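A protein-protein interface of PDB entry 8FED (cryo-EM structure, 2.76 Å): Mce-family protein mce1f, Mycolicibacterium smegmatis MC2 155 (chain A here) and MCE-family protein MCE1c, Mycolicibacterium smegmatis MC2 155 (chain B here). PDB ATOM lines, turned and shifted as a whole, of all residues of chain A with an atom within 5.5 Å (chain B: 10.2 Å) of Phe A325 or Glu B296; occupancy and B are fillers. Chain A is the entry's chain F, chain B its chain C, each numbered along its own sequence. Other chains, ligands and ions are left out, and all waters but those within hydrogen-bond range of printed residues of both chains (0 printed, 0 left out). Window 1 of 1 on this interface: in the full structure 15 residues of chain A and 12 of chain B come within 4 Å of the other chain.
The side-chain sulfur of Cys A348 is disulfide-bonded to the side-chain sulfur of Cys A321, 2.0 Å away. O of Gly A324 sits at hydrogen-bond distance from N of Tyr A347, 3.3 Å away. OG of Ser B300 sits close to NZ of Lys B305, 3.3 Å away. The guanidinium group (NH2) of Arg A362 is in hydrogen-bond range of the backbone carbonyl oxygen (O) of Ala A357, 2.5 Å away.
Glu B296 touches Phe A325 (CG to CZ, 3.7 Å). O of Leu A346 touches CB of Ser B293, 3.4 Å away. Glu B296 touches Tyr A347. CB of Cys A348 touches OE2 of Glu B296, at 3.2 Å. Ser B300 touches Ala A357. CA of Gly A360 touches OE2 of Glu B296, 3.2 Å away. Gly A360 touches Ala B299. Tyr A364 touches Ala B295 (OH to CB, 3.3 Å).
Printed residues of chain B within 4 Å of Phe A325: Glu B296. Leu A346 touches one residue of chain B. Printed residues of chain B within 4 Å of Tyr A347: Glu B296 (3.6 Å). Of chain B, only Glu B296 (3.2 Å) comes within 4 Å of Cys A348. Of chain B, only Glu B296 (3.2 Å) and Ala B299 (3.7 Å) come within 4 Å of Gly A360. Ala A361 touches one residue of chain B. Printed residues of chain A within 4 Å of Ser B293: Leu A346. Printed residues of chain A within 4 Å of Ala B295: Tyr A364 (3.3 Å). Of chain A, only Phe A325 (3.7 Å), Tyr A347 (3.6 Å), Cys A348 (3.2 Å), Gly A360 (3.2 Å) and Ala A361 (3.0 Å) come within 4 Å of Glu B296. Leu B298 touches none of the printed residues of chain A. Of the printed residues of chain A, Ser B300 touches Ala A357. Lys B305 touches none of the printed residues of chain A.
Of the 17 printed residues of chain A, 8 touch a printed residue of chain B. Among the printed residues, 9 pairs touch across the chains. Among the printed residues, no Asp or Glu carboxylate lies within 4 Å of a Lys or Arg side-chain nitrogen of the other chain.
N of Ala A361 is in hydrogen-bond range of OE1 of Glu B296, at 3.0 Å.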
ATOM      1  N   CYS A 321      16.254  -3.769  34.147  1.00  0.00           N
ATOM      2  CA  CYS A 321      15.035  -3.519  33.385  1.00  0.00           C
ATOM      3  C   CYS A 321      14.247  -4.818  33.295  1.00  0.00           C
ATOM      4  O   CYS A 321      14.684  -5.775  32.650  1.00  0.00           O
ATOM      5  CB  CYS A 321      15.326  -2.955  31.996  1.00  0.00           C
ATOM      6  SG  CYS A 321      16.780  -3.571  31.129  1.00  0.00           S
ATOM      7  N   LEU A 322      13.089  -4.849  33.947  1.00  0.00           N
ATOM      8  CA  LEU A 322      12.158  -5.962  33.850  1.00  0.00           C
ATOM      9  C   LEU A 322      11.117  -5.745  32.759  1.00  0.00           C
ATOM     10  O   LEU A 322      10.162  -6.522  32.665  1.00  0.00           O
ATOM     11  CB  LEU A 322      11.468  -6.188  35.195  1.00  0.00           C
ATOM     12  CG  LEU A 322      12.391  -6.234  36.413  1.00  0.00           C
ATOM     13  CD1 LEU A 322      11.604  -6.549  37.671  1.00  0.00           C
ATOM     14  CD2 LEU A 322      13.497  -7.248  36.207  1.00  0.00           C
ATOM     15  N   THR A 323      11.279  -4.703  31.948  1.00  0.00           N
ATOM     16  CA  THR A 323      10.371  -4.427  30.844  1.00  0.00           C
ATOM     17  C   THR A 323      10.768  -5.266  29.637  1.00  0.00           C
ATOM     18  O   THR A 323      11.868  -5.108  29.097  1.00  0.00           O
ATOM     19  CB  THR A 323      10.388  -2.942  30.494  1.00  0.00           C
ATOM     20  OG1 THR A 323      11.726  -2.541  30.175  1.00  0.00           O
ATOM     21  CG2 THR A 323       9.880  -2.115  31.661  1.00  0.00           C
ATOM     22  N   GLY A 324       9.874  -6.150  29.210  1.00  0.00           N
ATOM     23  CA  GLY A 324      10.146  -7.032  28.099  1.00  0.00           C
ATOM     24  C   GLY A 324      10.629  -8.413  28.470  1.00  0.00           C
ATOM     25  O   GLY A 324      11.017  -9.171  27.576  1.00  0.00           O
ATOM     26  N   PHE A 325      10.619  -8.763  29.748  1.00  0.00           N
ATOM     27  CA  PHE A 325      11.035 -10.076  30.214  1.00  0.00           C
ATOM     28  C   PHE A 325       9.835 -10.784  30.839  1.00  0.00           C
ATOM     29  O   PHE A 325       8.696 -10.320  30.742  1.00  0.00           O
ATOM     30  CB  PHE A 325      12.206  -9.952  31.192  1.00  0.00           C
ATOM     31  CG  PHE A 325      13.472  -9.455  30.556  1.00  0.00           C
ATOM     32  CD1 PHE A 325      14.305 -10.320  29.871  1.00  0.00           C
ATOM     33  CD2 PHE A 325      13.830  -8.122  30.644  1.00  0.00           C
ATOM     34  CE1 PHE A 325      15.468  -9.863  29.284  1.00  0.00           C
ATOM     35  CE2 PHE A 325      14.993  -7.663  30.061  1.00  0.00           C
ATOM     36  CZ  PHE A 325      15.812  -8.534  29.383  1.00  0.00           C
ATOM     37  N   LEU A 326      10.099 -11.926  31.464  1.00  0.00           N
ATOM     38  CA  LEU A 326       9.029 -12.753  32.000  1.00  0.00           C
ATOM     39  C   LEU A 326       8.274 -11.998  33.092  1.00  0.00           C
ATOM     40  O   LEU A 326       8.879 -11.214  33.834  1.00  0.00           O
ATOM     41  CB  LEU A 326       9.601 -14.057  32.560  1.00  0.00           C
ATOM     42  CG  LEU A 326       8.703 -15.292  32.581  1.00  0.00           C
ATOM     43  CD1 LEU A 326       8.346 -15.712  31.165  1.00  0.00           C
ATOM     44  CD2 LEU A 326       9.369 -16.434  33.334  1.00  0.00           C
ATOM     45  N   PRO A 327       6.957 -12.177  33.196  1.00  0.00           N
ATOM     46  CA  PRO A 327       6.204 -11.524  34.272  1.00  0.00           C
ATOM     47  C   PRO A 327       6.683 -11.970  35.644  1.00  0.00           C
ATOM     48  O   PRO A 327       7.122 -13.105  35.835  1.00  0.00           O
ATOM     49  CB  PRO A 327       4.760 -11.967  34.013  1.00  0.00           C
ATOM     50  CG  PRO A 327       4.719 -12.258  32.558  1.00  0.00           C
ATOM     51  CD  PRO A 327       6.066 -12.831  32.222  1.00  0.00           C
ATOM     52  N   LEU A 346      12.476 -11.848  24.252  1.00  0.00           N
ATOM     53  CA  LEU A 346      12.600 -11.173  25.538  1.00  0.00           C
ATOM     54  C   LEU A 346      13.889 -10.363  25.552  1.00  0.00           C
ATOM     55  O   LEU A 346      14.976 -10.930  25.405  1.00  0.00           O
ATOM     56  CB  LEU A 346      12.592 -12.177  26.691  1.00  0.00           C
ATOM     57  CG  LEU A 346      11.415 -13.147  26.791  1.00  0.00           C
ATOM     58  CD1 LEU A 346      11.561 -14.038  28.011  1.00  0.00           C
ATOM     59  CD2 LEU A 346      10.098 -12.398  26.831  1.00  0.00           C
ATOM     60  N   TYR A 347      13.767  -9.050  25.733  1.00  0.00           N
ATOM     61  CA  TYR A 347      14.930  -8.199  25.948  1.00  0.00           C
ATOM     62  C   TYR A 347      14.476  -6.883  26.566  1.00  0.00           C
ATOM     63  O   TYR A 347      13.280  -6.606  26.686  1.00  0.00           O
ATOM     64  CB  TYR A 347      15.720  -7.965  24.652  1.00  0.00           C
ATOM     65  CG  TYR A 347      15.050  -7.082  23.625  1.00  0.00           C
ATOM     66  CD1 TYR A 347      14.075  -7.587  22.777  1.00  0.00           C
ATOM     67  CD2 TYR A 347      15.421  -5.752  23.478  1.00  0.00           C
ATOM     68  CE1 TYR A 347      13.472  -6.787  21.826  1.00  0.00           C
ATOM     69  CE2 TYR A 347      14.822  -4.943  22.531  1.00  0.00           C
ATOM     70  CZ  TYR A 347      13.847  -5.466  21.710  1.00  0.00           C
ATOM     71  OH  TYR A 347      13.249  -4.668  20.764  1.00  0.00           O
ATOM     72  N   CYS A 348      15.460  -6.084  26.974  1.00  0.00           N
ATOM     73  CA  CYS A 348      15.230  -4.815  27.664  1.00  0.00           C
ATOM     74  C   CYS A 348      14.524  -3.841  26.727  1.00  0.00           C
ATOM     75  O   CYS A 348      15.125  -3.340  25.771  1.00  0.00           O
ATOM     76  CB  CYS A 348      16.566  -4.260  28.150  1.00  0.00           C
ATOM     77  SG  CYS A 348      16.563  -2.824  29.250  1.00  0.00           S
ATOM     78  N   LYS A 349      13.248  -3.570  27.002  1.00  0.00           N
ATOM     79  CA  LYS A 349      12.372  -2.792  26.126  1.00  0.00           C
ATOM     80  C   LYS A 349      12.240  -1.343  26.578  1.00  0.00           C
ATOM     81  O   LYS A 349      11.169  -0.744  26.457  1.00  0.00           O
ATOM     82  CB  LYS A 349      10.995  -3.442  26.051  1.00  0.00           C
ATOM     83  CG  LYS A 349      10.943  -4.789  25.362  1.00  0.00           C
ATOM     84  CD  LYS A 349      11.059  -4.660  23.857  1.00  0.00           C
ATOM     85  CE  LYS A 349      10.371  -5.827  23.167  1.00  0.00           C
ATOM     86  NZ  LYS A 349      10.835  -7.140  23.688  1.00  0.00           N
ATOM     87  N   ALA A 357      21.274   0.330  30.354  1.00  0.00           N
ATOM     88  CA  ALA A 357      21.297  -0.652  29.265  1.00  0.00           C
ATOM     89  C   ALA A 357      21.527  -0.002  27.904  1.00  0.00           C
ATOM     90  O   ALA A 357      20.798  -0.247  26.941  1.00  0.00           O
ATOM     91  CB  ALA A 357      20.015  -1.482  29.259  1.00  0.00           C
ATOM     92  N   GLY A 360      22.371  -2.606  25.109  1.00  0.00           N
ATOM     93  CA  GLY A 360      21.452  -3.719  25.035  1.00  0.00           C
ATOM     94  C   GLY A 360      21.119  -4.079  23.599  1.00  0.00           C
ATOM     95  O   GLY A 360      21.699  -3.563  22.643  1.00  0.00           O
ATOM     96  N   ALA A 361      20.163  -5.002  23.456  1.00  0.00           N
ATOM     97  CA  ALA A 361      19.802  -5.495  22.129  1.00  0.00           C
ATOM     98  C   ALA A 361      19.239  -4.384  21.255  1.00  0.00           C
ATOM     99  O   ALA A 361      19.542  -4.312  20.059  1.00  0.00           O
ATOM    100  CB  ALA A 361      18.798  -6.640  22.242  1.00  0.00           C
ATOM    101  N   ARG A 362      18.427  -3.500  21.838  1.00  0.00           N
ATOM    102  CA  ARG A 362      17.789  -2.413  21.104  1.00  0.00           C
ATOM    103  C   ARG A 362      18.774  -1.474  20.420  1.00  0.00           C
ATOM    104  O   ARG A 362      18.338  -0.604  19.659  1.00  0.00           O
ATOM    105  CB  ARG A 362      16.907  -1.607  22.053  1.00  0.00           C
ATOM    106  CG  ARG A 362      17.648  -1.164  23.294  1.00  0.00           C
ATOM    107  CD  ARG A 362      16.890  -0.115  24.071  1.00  0.00           C
ATOM    108  NE  ARG A 362      17.634   0.302  25.253  1.00  0.00           N
ATOM    109  CZ  ARG A 362      18.570   1.239  25.261  1.00  0.00           C
ATOM    110  NH1 ARG A 362      18.919   1.878  24.158  1.00  0.00           N
ATOM    111  NH2 ARG A 362      19.174   1.543  26.405  1.00  0.00           N
ATOM    112  N   TYR A 364      21.818  -2.762  18.889  1.00  0.00           N
ATOM    113  CA  TYR A 364      22.710  -3.499  18.004  1.00  0.00           C
ATOM    114  C   TYR A 364      22.610  -2.923  16.598  1.00  0.00           C
ATOM    115  O   TYR A 364      21.502  -2.850  16.053  1.00  0.00           O
ATOM    116  CB  TYR A 364      22.357  -4.981  17.984  1.00  0.00           C
ATOM    117  CG  TYR A 364      22.607  -5.716  19.279  1.00  0.00           C
ATOM    118  CD1 TYR A 364      23.440  -5.191  20.254  1.00  0.00           C
ATOM    119  CD2 TYR A 364      22.019  -6.949  19.518  1.00  0.00           C
ATOM    120  CE1 TYR A 364      23.663  -5.865  21.436  1.00  0.00           C
ATOM    121  CE2 TYR A 364      22.245  -7.632  20.691  1.00  0.00           C
ATOM    122  CZ  TYR A 364      23.068  -7.086  21.646  1.00  0.00           C
ATOM    123  OH  TYR A 364      23.293  -7.760  22.821  1.00  0.00           O
ATOM    124  N   ASP A 399       4.613  -3.977  32.854  1.00  0.00           N
ATOM    125  CA  ASP A 399       4.001  -4.440  31.600  1.00  0.00           C
ATOM    126  C   ASP A 399       5.003  -4.944  30.561  1.00  0.00           C
ATOM    127  O   ASP A 399       5.909  -5.712  30.883  1.00  0.00           O
ATOM    128  CB  ASP A 399       3.120  -3.335  30.985  1.00  0.00           C
ATOM    129  CG  ASP A 399       3.859  -2.024  30.784  1.00  0.00           C
ATOM    130  OD1 ASP A 399       4.742  -1.960  29.904  1.00  0.00           O
ATOM    131  OD2 ASP A 399       3.552  -1.053  31.508  1.00  0.00           O
ATOM    132  N   LYS B 289      17.625 -17.991  19.700  1.00  0.00           N
ATOM    133  CA  LYS B 289      16.479 -17.423  20.393  1.00  0.00           C
ATOM    134  C   LYS B 289      16.794 -16.968  21.812  1.00  0.00           C
ATOM    135  O   LYS B 289      15.878 -16.548  22.526  1.00  0.00           O
ATOM    136  CB  LYS B 289      15.328 -18.433  20.423  1.00  0.00           C
ATOM    137  CG  LYS B 289      15.594 -19.645  21.293  1.00  0.00           C
ATOM    138  CD  LYS B 289      14.510 -20.694  21.120  1.00  0.00           C
ATOM    139  CE  LYS B 289      13.165 -20.184  21.598  1.00  0.00           C
ATOM    140  NZ  LYS B 289      12.107 -21.221  21.452  1.00  0.00           N
ATOM    141  N   PHE B 290      18.053 -17.043  22.246  1.00  0.00           N
ATOM    142  CA  PHE B 290      18.402 -16.606  23.590  1.00  0.00           C
ATOM    143  C   PHE B 290      19.690 -15.804  23.662  1.00  0.00           C
ATOM    144  O   PHE B 290      20.042 -15.347  24.754  1.00  0.00           O
ATOM    145  CB  PHE B 290      18.513 -17.816  24.538  1.00  0.00           C
ATOM    146  CG  PHE B 290      19.884 -18.445  24.575  1.00  0.00           C
ATOM    147  CD1 PHE B 290      20.317 -19.258  23.546  1.00  0.00           C
ATOM    148  CD2 PHE B 290      20.733 -18.235  25.648  1.00  0.00           C
ATOM    149  CE1 PHE B 290      21.572 -19.838  23.582  1.00  0.00           C
ATOM    150  CE2 PHE B 290      21.983 -18.814  25.685  1.00  0.00           C
ATOM    151  CZ  PHE B 290      22.402 -19.614  24.652  1.00  0.00           C
ATOM    152  N   ILE B 291      20.397 -15.604  22.550  1.00  0.00           N
ATOM    153  CA  ILE B 291      21.671 -14.895  22.607  1.00  0.00           C
ATOM    154  C   ILE B 291      21.456 -13.423  22.947  1.00  0.00           C
ATOM    155  O   ILE B 291      22.218 -12.837  23.727  1.00  0.00           O
ATOM    156  CB  ILE B 291      22.444 -15.087  21.289  1.00  0.00           C
ATOM    157  CG1 ILE B 291      23.736 -14.275  21.292  1.00  0.00           C
ATOM    158  CG2 ILE B 291      21.576 -14.749  20.087  1.00  0.00           C
ATOM    159  CD1 ILE B 291      24.565 -14.485  20.057  1.00  0.00           C
ATOM    160  N   THR B 292      20.411 -12.805  22.386  1.00  0.00           N
ATOM    161  CA  THR B 292      20.094 -11.424  22.736  1.00  0.00           C
ATOM    162  C   THR B 292      19.678 -11.308  24.197  1.00  0.00           C
ATOM    163  O   THR B 292      20.110 -10.388  24.901  1.00  0.00           O
ATOM    164  CB  THR B 292      18.988 -10.888  21.829  1.00  0.00           C
ATOM    165  OG1 THR B 292      17.766 -11.586  22.099  1.00  0.00           O
ATOM    166  CG2 THR B 292      19.353 -11.080  20.370  1.00  0.00           C
ATOM    167  N   SER B 293      18.843 -12.238  24.668  1.00  0.00           N
ATOM    168  CA  SER B 293      18.400 -12.207  26.058  1.00  0.00           C
ATOM    169  C   SER B 293      19.568 -12.391  27.019  1.00  0.00           C
ATOM    170  O   SER B 293      19.619 -11.749  28.074  1.00  0.00           O
ATOM    171  CB  SER B 293      17.337 -13.279  26.291  1.00  0.00           C
ATOM    172  OG  SER B 293      16.934 -13.308  27.648  1.00  0.00           O
ATOM    173  N   LEU B 294      20.513 -13.271  26.677  1.00  0.00           N
ATOM    174  CA  LEU B 294      21.666 -13.476  27.548  1.00  0.00           C
ATOM    175  C   LEU B 294      22.606 -12.279  27.519  1.00  0.00           C
ATOM    176  O   LEU B 294      23.117 -11.859  28.563  1.00  0.00           O
ATOM    177  CB  LEU B 294      22.416 -14.745  27.141  1.00  0.00           C
ATOM    178  CG  LEU B 294      22.897 -15.647  28.278  1.00  0.00           C
ATOM    179  CD1 LEU B 294      21.726 -16.292  28.988  1.00  0.00           C
ATOM    180  CD2 LEU B 294      23.864 -16.697  27.767  1.00  0.00           C
ATOM    181  N   ALA B 295      22.850 -11.714  26.335  1.00  0.00           N
ATOM    182  CA  ALA B 295      23.688 -10.528  26.229  1.00  0.00           C
ATOM    183  C   ALA B 295      23.032  -9.282  26.803  1.00  0.00           C
ATOM    184  O   ALA B 295      23.712  -8.261  26.947  1.00  0.00           O
ATOM    185  CB  ALA B 295      24.062 -10.269  24.771  1.00  0.00           C
ATOM    186  N   GLU B 296      21.729  -9.326  27.090  1.00  0.00           N
ATOM    187  CA  GLU B 296      21.080  -8.169  27.695  1.00  0.00           C
ATOM    188  C   GLU B 296      21.635  -7.859  29.079  1.00  0.00           C
ATOM    189  O   GLU B 296      21.848  -6.689  29.416  1.00  0.00           O
ATOM    190  CB  GLU B 296      19.571  -8.403  27.773  1.00  0.00           C
ATOM    191  CG  GLU B 296      18.758  -7.133  27.651  1.00  0.00           C
ATOM    192  CD  GLU B 296      18.955  -6.460  26.310  1.00  0.00           C
ATOM    193  OE1 GLU B 296      19.172  -7.181  25.318  1.00  0.00           O
ATOM    194  OE2 GLU B 296      18.908  -5.216  26.246  1.00  0.00           O
ATOM    195  N   ALA B 297      21.871  -8.891  29.899  1.00  0.00           N
ATOM    196  CA  ALA B 297      22.233  -8.658  31.296  1.00  0.00           C
ATOM    197  C   ALA B 297      23.540  -7.889  31.414  1.00  0.00           C
ATOM    198  O   ALA B 297      23.656  -6.954  32.213  1.00  0.00           O
ATOM    199  CB  ALA B 297      22.327  -9.987  32.044  1.00  0.00           C
ATOM    200  N   LEU B 298      24.530  -8.271  30.619  1.00  0.00           N
ATOM    201  CA  LEU B 298      25.843  -7.631  30.599  1.00  0.00           C
ATOM    202  C   LEU B 298      25.920  -6.507  29.558  1.00  0.00           C
ATOM    203  O   LEU B 298      26.766  -6.467  28.670  1.00  0.00           O
ATOM    204  CB  LEU B 298      26.899  -8.724  30.442  1.00  0.00           C
ATOM    205  CG  LEU B 298      27.027  -9.706  29.262  1.00  0.00           C
ATOM    206  CD1 LEU B 298      27.690  -9.243  27.990  1.00  0.00           C
ATOM    207  CD2 LEU B 298      27.674 -10.980  29.776  1.00  0.00           C
ATOM    208  N   ALA B 299      25.031  -5.529  29.734  1.00  0.00           N
ATOM    209  CA  ALA B 299      24.931  -4.402  28.813  1.00  0.00           C
ATOM    210  C   ALA B 299      24.970  -3.058  29.534  1.00  0.00           C
ATOM    211  O   ALA B 299      25.418  -2.059  28.965  1.00  0.00           O
ATOM    212  CB  ALA B 299      23.653  -4.505  27.979  1.00  0.00           C
ATOM    213  N   SER B 300      24.498  -3.030  30.785  1.00  0.00           N
ATOM    214  CA  SER B 300      24.381  -1.774  31.522  1.00  0.00           C
ATOM    215  C   SER B 300      25.741  -1.131  31.765  1.00  0.00           C
ATOM    216  O   SER B 300      25.905   0.080  31.580  1.00  0.00           O
ATOM    217  CB  SER B 300      23.656  -2.012  32.847  1.00  0.00           C
ATOM    218  OG  SER B 300      22.345  -2.501  32.633  1.00  0.00           O
ATOM    219  N   GLY B 301      26.728  -1.921  32.180  1.00  0.00           N
ATOM    220  CA  GLY B 301      28.036  -1.389  32.485  1.00  0.00           C
ATOM    221  C   GLY B 301      29.142  -2.393  32.244  1.00  0.00           C
ATOM    222  O   GLY B 301      28.925  -3.462  31.663  1.00  0.00           O
ATOM    223  N   TYR B 303      30.303  -4.841  33.683  1.00  0.00           N
ATOM    224  CA  TYR B 303      30.005  -5.888  34.657  1.00  0.00           C
ATOM    225  C   TYR B 303      28.817  -6.678  34.118  1.00  0.00           C
ATOM    226  O   TYR B 303      28.369  -6.456  32.987  1.00  0.00           O
ATOM    227  CB  TYR B 303      29.728  -5.301  36.043  1.00  0.00           C
ATOM    228  CG  TYR B 303      29.096  -3.926  36.019  1.00  0.00           C
ATOM    229  CD1 TYR B 303      27.754  -3.757  35.711  1.00  0.00           C
ATOM    230  CD2 TYR B 303      29.846  -2.795  36.307  1.00  0.00           C
ATOM    231  CE1 TYR B 303      27.178  -2.501  35.692  1.00  0.00           C
ATOM    232  CE2 TYR B 303      29.281  -1.538  36.286  1.00  0.00           C
ATOM    233  CZ  TYR B 303      27.950  -1.396  35.979  1.00  0.00           C
ATOM    234  OH  TYR B 303      27.392  -0.142  35.961  1.00  0.00           O
ATOM    235  N   PHE B 304      28.306  -7.606  34.921  1.00  0.00           N
ATOM    236  CA  PHE B 304      27.087  -8.327  34.582  1.00  0.00           C
ATOM    237  C   PHE B 304      26.268  -8.541  35.844  1.00  0.00           C
ATOM    238  O   PHE B 304      26.811  -8.923  36.883  1.00  0.00           O
ATOM    239  CB  PHE B 304      27.401  -9.668  33.900  1.00  0.00           C
ATOM    240  CG  PHE B 304      28.128 -10.650  34.773  1.00  0.00           C
ATOM    241  CD1 PHE B 304      29.498 -10.571  34.934  1.00  0.00           C
ATOM    242  CD2 PHE B 304      27.444 -11.670  35.413  1.00  0.00           C
ATOM    243  CE1 PHE B 304      30.167 -11.473  35.731  1.00  0.00           C
ATOM    244  CE2 PHE B 304      28.111 -12.577  36.207  1.00  0.00           C
ATOM    245  CZ  PHE B 304      29.471 -12.477  36.368  1.00  0.00           C
ATOM    246  N   LYS B 305      24.968  -8.288  35.757  1.00  0.00           N
ATOM    247  CA  LYS B 305      24.114  -8.410  36.926  1.00  0.00           C
ATOM    248  C   LYS B 305      23.878  -9.873  37.275  1.00  0.00           C
ATOM    249  O   LYS B 305      23.886 -10.751  36.410  1.00  0.00           O
ATOM    250  CB  LYS B 305      22.787  -7.700  36.689  1.00  0.00           C
ATOM    251  CG  LYS B 305      22.944  -6.264  36.234  1.00  0.00           C
ATOM    252  CD  LYS B 305      21.603  -5.580  36.085  1.00  0.00           C
ATOM    253  CE  LYS B 305      21.739  -4.319  35.264  1.00  0.00           C
ATOM    254  NZ  LYS B 305      22.890  -3.513  35.737  1.00  0.00           N
ATOM    255  N   VAL B 306      23.669 -10.130  38.565  1.00  0.00           N
ATOM    256  CA  VAL B 306      23.393 -11.468  39.076  1.00  0.00           C
ATOM    257  C   VAL B 306      22.329 -11.367  40.158  1.00  0.00           C
ATOM    258  O   VAL B 306      22.296 -10.399  40.924  1.00  0.00           O
ATOM    259  CB  VAL B 306      24.660 -12.151  39.631  1.00  0.00           C
ATOM    260  CG1 VAL B 306      25.547 -12.624  38.506  1.00  0.00           C
ATOM    261  CG2 VAL B 306      25.421 -11.203  40.537  1.00  0.00           C
